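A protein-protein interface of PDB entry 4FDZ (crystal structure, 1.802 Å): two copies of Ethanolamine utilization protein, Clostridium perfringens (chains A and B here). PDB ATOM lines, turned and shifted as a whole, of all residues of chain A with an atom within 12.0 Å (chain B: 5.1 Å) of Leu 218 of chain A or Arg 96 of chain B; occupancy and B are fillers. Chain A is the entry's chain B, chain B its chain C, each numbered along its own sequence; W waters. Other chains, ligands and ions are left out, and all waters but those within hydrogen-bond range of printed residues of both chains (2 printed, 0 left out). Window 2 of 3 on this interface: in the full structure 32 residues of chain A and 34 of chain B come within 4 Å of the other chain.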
ATOM      1  N   TYR A 159      17.674  20.176   1.679  1.00  0.00           N
ATOM      2  CA  TYR A 159      19.120  20.395   1.777  1.00  0.00           C
ATOM      3  C   TYR A 159      19.438  21.753   2.421  1.00  0.00           C
ATOM      4  O   TYR A 159      20.291  21.851   3.311  1.00  0.00           O
ATOM      5  CB  TYR A 159      19.706  20.324   0.370  1.00  0.00           C
ATOM      6  CG  TYR A 159      21.217  20.409   0.269  1.00  0.00           C
ATOM      7  CD1 TYR A 159      22.014  19.280   0.425  1.00  0.00           C
ATOM      8  CD2 TYR A 159      21.839  21.614  -0.010  1.00  0.00           C
ATOM      9  CE1 TYR A 159      23.400  19.363   0.312  1.00  0.00           C
ATOM     10  CE2 TYR A 159      23.212  21.700  -0.123  1.00  0.00           C
ATOM     11  CZ  TYR A 159      23.980  20.583   0.031  1.00  0.00           C
ATOM     12  OH  TYR A 159      25.343  20.716  -0.086  1.00  0.00           O
ATOM     13  N   SER A 209      23.782  26.573  -4.298  1.00  0.00           N
ATOM     14  CA  SER A 209      24.758  25.494  -4.416  1.00  0.00           C
ATOM     15  C   SER A 209      24.169  24.276  -5.135  1.00  0.00           C
ATOM     16  O   SER A 209      24.835  23.646  -5.954  1.00  0.00           O
ATOM     17  CB  SER A 209      25.277  25.096  -3.027  1.00  0.00           C
ATOM     18  OG  SER A 209      26.199  24.020  -3.097  1.00  0.00           O
ATOM     19  N   ASN A 213      25.076  22.555  -8.863  1.00  0.00           N
ATOM     20  CA  ASN A 213      25.619  21.200  -8.827  1.00  0.00           C
ATOM     21  C   ASN A 213      24.534  20.197  -8.436  1.00  0.00           C
ATOM     22  O   ASN A 213      24.572  19.603  -7.353  1.00  0.00           O
ATOM     23  CB  ASN A 213      26.785  21.144  -7.839  1.00  0.00           C
ATOM     24  CG  ASN A 213      27.383  19.768  -7.712  1.00  0.00           C
ATOM     25  OD1 ASN A 213      27.327  18.966  -8.641  1.00  0.00           O
ATOM     26  ND2 ASN A 213      27.960  19.482  -6.549  1.00  0.00           N
ATOM     27  N   PRO A 214      23.560  20.002  -9.325  1.00  0.00           N
ATOM     28  CA  PRO A 214      22.343  19.305  -8.868  1.00  0.00           C
ATOM     29  C   PRO A 214      22.520  17.814  -8.636  1.00  0.00           C
ATOM     30  O   PRO A 214      21.780  17.243  -7.830  1.00  0.00           O
ATOM     31  CB  PRO A 214      21.325  19.569  -9.985  1.00  0.00           C
ATOM     32  CG  PRO A 214      22.109  20.103 -11.152  1.00  0.00           C
ATOM     33  CD  PRO A 214      23.390  20.674 -10.623  1.00  0.00           C
ATOM     34  N   LEU A 215      23.483  17.192  -9.315  1.00  0.00           N
ATOM     35  CA  LEU A 215      23.641  15.741  -9.234  1.00  0.00           C
ATOM     36  C   LEU A 215      24.842  15.303  -8.390  1.00  0.00           C
ATOM     37  O   LEU A 215      25.064  14.100  -8.206  1.00  0.00           O
ATOM     38  CB  LEU A 215      23.776  15.150 -10.643  1.00  0.00           C
ATOM     39  CG  LEU A 215      22.616  15.338 -11.623  1.00  0.00           C
ATOM     40  CD1 LEU A 215      23.052  14.886 -13.016  1.00  0.00           C
ATOM     41  CD2 LEU A 215      21.386  14.565 -11.174  1.00  0.00           C
ATOM     42  N   GLY A 216      25.615  16.262  -7.881  1.00  0.00           N
ATOM     43  CA  GLY A 216      26.856  15.949  -7.170  1.00  0.00           C
ATOM     44  C   GLY A 216      26.662  15.519  -5.720  1.00  0.00           C
ATOM     45  O   GLY A 216      26.124  16.269  -4.923  1.00  0.00           O
ATOM     46  N   PHE A 217      27.109  14.315  -5.362  1.00  0.00           N
ATOM     47  CA  PHE A 217      26.942  13.841  -3.987  1.00  0.00           C
ATOM     48  C   PHE A 217      28.097  12.988  -3.455  1.00  0.00           C
ATOM     49  O   PHE A 217      28.021  12.471  -2.339  1.00  0.00           O
ATOM     50  CB  PHE A 217      25.623  13.060  -3.860  1.00  0.00           C
ATOM     51  CG  PHE A 217      25.615  11.735  -4.569  1.00  0.00           C
ATOM     52  CD1 PHE A 217      25.423  11.660  -5.937  1.00  0.00           C
ATOM     53  CD2 PHE A 217      25.780  10.556  -3.855  1.00  0.00           C
ATOM     54  CE1 PHE A 217      25.409  10.434  -6.587  1.00  0.00           C
ATOM     55  CE2 PHE A 217      25.764   9.324  -4.494  1.00  0.00           C
ATOM     56  CZ  PHE A 217      25.583   9.260  -5.863  1.00  0.00           C
ATOM     57  N   LEU A 218      29.164  12.845  -4.234  1.00  0.00           N
ATOM     58  CA  LEU A 218      30.186  11.840  -3.933  1.00  0.00           C
ATOM     59  C   LEU A 218      31.326  12.352  -3.067  1.00  0.00           C
ATOM     60  O   LEU A 218      32.168  11.561  -2.625  1.00  0.00           O
ATOM     61  CB  LEU A 218      30.772  11.262  -5.223  1.00  0.00           C
ATOM     62  CG  LEU A 218      29.836  10.413  -6.070  1.00  0.00           C
ATOM     63  CD1 LEU A 218      30.524  10.029  -7.379  1.00  0.00           C
ATOM     64  CD2 LEU A 218      29.394   9.163  -5.307  1.00  0.00           C
ATOM     65  N   GLU A 219      31.367  13.658  -2.833  1.00  0.00           N
ATOM     66  CA  GLU A 219      32.457  14.255  -2.068  1.00  0.00           C
ATOM     67  C   GLU A 219      32.464  13.775  -0.618  1.00  0.00           C
ATOM     68  O   GLU A 219      31.419  13.429  -0.064  1.00  0.00           O
ATOM     69  CB  GLU A 219      32.377  15.785  -2.106  1.00  0.00           C
ATOM     70  CG  GLU A 219      31.159  16.381  -1.416  1.00  0.00           C
ATOM     71  CD  GLU A 219      29.940  16.461  -2.322  1.00  0.00           C
ATOM     72  OE1 GLU A 219      29.963  15.860  -3.422  1.00  0.00           O
ATOM     73  OE2 GLU A 219      28.962  17.133  -1.934  1.00  0.00           O
ATOM     74  N   HIS A 220      33.647  13.759  -0.007  1.00  0.00           N
ATOM     75  CA  HIS A 220      33.783  13.344   1.386  1.00  0.00           C
ATOM     76  C   HIS A 220      32.841  14.113   2.309  1.00  0.00           C
ATOM     77  O   HIS A 220      32.747  15.344   2.249  1.00  0.00           O
ATOM     78  CB  HIS A 220      35.221  13.527   1.877  1.00  0.00           C
ATOM     79  CG  HIS A 220      35.364  13.426   3.366  1.00  0.00           C
ATOM     80  ND1 HIS A 220      35.217  12.239   4.050  1.00  0.00           N
ATOM     81  CD2 HIS A 220      35.631  14.369   4.302  1.00  0.00           C
ATOM     82  CE1 HIS A 220      35.392  12.453   5.343  1.00  0.00           C
ATOM     83  NE2 HIS A 220      35.647  13.738   5.523  1.00  0.00           N
ATOM     84  N   HIS A 221      32.160  13.368   3.173  1.00  0.00           N
ATOM     85  CA  HIS A 221      31.242  13.943   4.145  1.00  0.00           C
ATOM     86  C   HIS A 221      31.661  13.564   5.563  1.00  0.00           C
ATOM     87  O   HIS A 221      32.045  12.419   5.824  1.00  0.00           O
ATOM     88  CB  HIS A 221      29.820  13.452   3.870  1.00  0.00           C
ATOM     89  CG  HIS A 221      29.095  14.241   2.821  1.00  0.00           C
ATOM     90  ND1 HIS A 221      28.420  15.411   3.101  1.00  0.00           N
ATOM     91  CD2 HIS A 221      28.939  14.026   1.492  1.00  0.00           C
ATOM     92  CE1 HIS A 221      27.882  15.882   1.990  1.00  0.00           C
ATOM     93  NE2 HIS A 221      28.182  15.061   1.000  1.00  0.00           N
ATOM     94  N   ILE B  15      23.328  14.606  -0.493  1.00  0.00           N
ATOM     95  CA  ILE B  15      23.437  13.947   0.804  1.00  0.00           C
ATOM     96  C   ILE B  15      23.483  14.991   1.915  1.00  0.00           C
ATOM     97  O   ILE B  15      24.095  16.052   1.763  1.00  0.00           O
ATOM     98  CB  ILE B  15      24.687  13.054   0.890  1.00  0.00           C
ATOM     99  CG1 ILE B  15      24.501  11.801   0.039  1.00  0.00           C
ATOM    100  CG2 ILE B  15      24.973  12.650   2.332  1.00  0.00           C
ATOM    101  CD1 ILE B  15      25.684  10.847   0.096  1.00  0.00           C
ATOM    102  N   PRO B  92      27.099   8.578   6.097  1.00  0.00           N
ATOM    103  CA  PRO B  92      27.104   9.011   4.700  1.00  0.00           C
ATOM    104  C   PRO B  92      27.505   7.892   3.744  1.00  0.00           C
ATOM    105  O   PRO B  92      27.004   7.866   2.629  1.00  0.00           O
ATOM    106  CB  PRO B  92      28.157  10.123   4.684  1.00  0.00           C
ATOM    107  CG  PRO B  92      28.211  10.613   6.101  1.00  0.00           C
ATOM    108  CD  PRO B  92      27.993   9.399   6.936  1.00  0.00           C
ATOM    109  N   ALA B  93      28.395   6.991   4.157  1.00  0.00           N
ATOM    110  CA  ALA B  93      28.818   5.919   3.260  1.00  0.00           C
ATOM    111  C   ALA B  93      27.637   5.026   2.857  1.00  0.00           C
ATOM    112  O   ALA B  93      27.490   4.654   1.692  1.00  0.00           O
ATOM    113  CB  ALA B  93      29.929   5.085   3.897  1.00  0.00           C
ATOM    114  N   GLU B  94      26.787   4.685   3.817  1.00  0.00           N
ATOM    115  CA  GLU B  94      25.654   3.814   3.516  1.00  0.00           C
ATOM    116  C   GLU B  94      24.643   4.534   2.638  1.00  0.00           C
ATOM    117  O   GLU B  94      24.079   3.949   1.707  1.00  0.00           O
ATOM    118  CB  GLU B  94      24.996   3.313   4.798  1.00  0.00           C
ATOM    119  CG  GLU B  94      25.822   2.245   5.538  1.00  0.00           C
ATOM    120  CD  GLU B  94      26.068   0.973   4.718  1.00  0.00           C
ATOM    121  OE1 GLU B  94      27.055   0.250   5.012  1.00  0.00           O
ATOM    122  OE2 GLU B  94      25.287   0.674   3.787  1.00  0.00           O
ATOM    123  N   VAL B  95      24.395   5.802   2.933  1.00  0.00           N
ATOM    124  CA  VAL B  95      23.452   6.565   2.120  1.00  0.00           C
ATOM    125  C   VAL B  95      23.966   6.707   0.687  1.00  0.00           C
ATOM    126  O   VAL B  95      23.219   6.596  -0.276  1.00  0.00           O
ATOM    127  CB  VAL B  95      23.192   7.944   2.720  1.00  0.00           C
ATOM    128  CG1 VAL B  95      22.616   8.866   1.661  1.00  0.00           C
ATOM    129  CG2 VAL B  95      22.252   7.808   3.901  1.00  0.00           C
ATOM    130  N   ARG B  96      25.259   6.951   0.562  1.00  0.00           N
ATOM    131  CA  ARG B  96      25.920   7.020  -0.729  1.00  0.00           C
ATOM    132  C   ARG B  96      25.717   5.721  -1.512  1.00  0.00           C
ATOM    133  O   ARG B  96      25.381   5.731  -2.695  1.00  0.00           O
ATOM    134  CB  ARG B  96      27.402   7.237  -0.453  1.00  0.00           C
ATOM    135  CG  ARG B  96      28.219   7.939  -1.483  1.00  0.00           C
ATOM    136  CD  ARG B  96      29.570   8.165  -0.819  1.00  0.00           C
ATOM    137  NE  ARG B  96      30.643   8.621  -1.693  1.00  0.00           N
ATOM    138  CZ  ARG B  96      31.284   7.851  -2.563  1.00  0.00           C
ATOM    139  NH1 ARG B  96      30.931   6.580  -2.720  1.00  0.00           N
ATOM    140  NH2 ARG B  96      32.265   8.363  -3.296  1.00  0.00           N
ATOM    141  N   SER B  97      25.914   4.592  -0.844  1.00  0.00           N
ATOM    142  CA  SER B  97      25.724   3.291  -1.474  1.00  0.00           C
ATOM    143  C   SER B  97      24.269   3.099  -1.917  1.00  0.00           C
ATOM    144  O   SER B  97      23.999   2.613  -3.024  1.00  0.00           O
ATOM    145  CB  SER B  97      26.147   2.188  -0.500  1.00  0.00           C
ATOM    146  OG  SER B  97      26.022   0.918  -1.092  1.00  0.00           O
ATOM    147  N   GLY B  98      23.332   3.483  -1.053  1.00  0.00           N
ATOM    148  CA  GLY B  98      21.919   3.424  -1.384  1.00  0.00           C
ATOM    149  C   GLY B  98      21.566   4.294  -2.587  1.00  0.00           C
ATOM    150  O   GLY B  98      20.808   3.881  -3.458  1.00  0.00           O
ATOM    151  N   LEU B  99      22.114   5.507  -2.643  1.00  0.00           N
ATOM    152  CA  LEU B  99      21.789   6.418  -3.741  1.00  0.00           C
ATOM    153  C   LEU B  99      22.351   5.899  -5.061  1.00  0.00           C
ATOM    154  O   LEU B  99      21.694   5.976  -6.103  1.00  0.00           O
ATOM    155  CB  LEU B  99      22.325   7.819  -3.468  1.00  0.00           C
ATOM    156  CG  LEU B  99      21.559   8.671  -2.463  1.00  0.00           C
ATOM    157  CD1 LEU B  99      22.346   9.943  -2.142  1.00  0.00           C
ATOM    158  CD2 LEU B  99      20.169   9.012  -2.970  1.00  0.00           C
ATOM    159  N   ASN B 100      23.562   5.365  -5.022  1.00  0.00           N
ATOM    160  CA  ASN B 100      24.145   4.784  -6.222  1.00  0.00           C
ATOM    161  C   ASN B 100      23.285   3.641  -6.765  1.00  0.00           C
ATOM    162  O   ASN B 100      23.060   3.548  -7.974  1.00  0.00           O
ATOM    163  CB  ASN B 100      25.581   4.325  -5.966  1.00  0.00           C
ATOM    164  CG  ASN B 100      26.580   5.467  -6.092  1.00  0.00           C
ATOM    165  OD1 ASN B 100      26.781   5.999  -7.178  1.00  0.00           O
ATOM    166  ND2 ASN B 100      27.199   5.858  -4.978  1.00  0.00           N
ATOM    167  N   ALA B 101      22.787   2.780  -5.879  1.00  0.00           N
ATOM    168  CA  ALA B 101      21.888   1.696  -6.311  1.00  0.00           C
ATOM    169  C   ALA B 101      20.577   2.231  -6.916  1.00  0.00           C
ATOM    170  O   ALA B 101      20.025   1.657  -7.871  1.00  0.00           O
ATOM    171  CB  ALA B 101      21.592   0.760  -5.140  1.00  0.00           C
HETATM  172  O   HOH W   1      29.541  11.160  -0.215  1.00  0.00           O
HETATM  173  O   HOH W   2      32.850   9.902  -0.730  1.00  0.00           O
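Among the printed residues, merely in contact across the chains: Tyr 159 of chain A with Ile 15 of chain B, Phe 217 of chain A with Ile 15 of chain B, Phe 217 of chain A with Leu 99 of chain B, Phe 217 of chain A with Asn 100 of chain B, Leu 218 of chain A with Asn 100 of chain B, His 221 of chain A with Ile 15 of chain B and His 221 of chain A with Pro 92 of chain B.
Water W2 lies within hydrogen-bond range of O of Leu 218 of chain A (2.6 Å) and NE of Arg 96 of chain B (2.7 Å). Water W1 lies within hydrogen-bond range of O of Phe 217 of chain A (2.9 Å), O of Glu 219 of chain A (2.9 Å) and NE of Arg 96 of chain B (3.1 Å).
O of Leu 218 of chain A is in hydrogen-bond range of NH2 of Arg 96 of chain B.
Hydrophobic or aromatic side chains of chain A that line the printed part of chain B: Tyr 159, Phe 217, Leu 218 and His 221. Along chain A the printed residues that touch a printed residue of chain B span positions 159 to 221. Printed residues of chain B that touch a printed residue of chain A: Ile 15, Pro 92, Arg 96, Leu 99 and Asn 100. Along chain B the printed residues that touch a printed residue of chain A span positions 15 to 100. Among the printed residues, 8 pairs touch across the chains.
Of the printed residues of chain B, Leu 218 of chain A touches Arg 96 (3.3 Å) and Asn 100 (3.98 Å). Arg 96 of chain B touches one residue of chain A. Of chain A, only His 221 comes within 4 Å of Pro 92 of chain B. No residue of chain A comes within 4 Å of Ser 97 of chain B. Leu 99 of chain B touches just one residue of chain A: Phe 217 (3.9 Å). Printed residues of chain B within 4 Å of Tyr 159 of chain A: Ile 15 (3.7 Å). Of the printed residues of chain A, Ile 15 of chain B touches Tyr 159 (3.7 Å), Phe 217 (3.7 Å) and His 221 (3.8 Å). His 220 of chain A touches none of the printed residues of chain B.
No position is printed for both chains.
The side-chain amide nitrogen (ND2) of Asn 100 of chain B sits at hydrogen-bond distance from the backbone carbonyl oxygen (O) of Arg 96 of chain B (2.9 Å).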
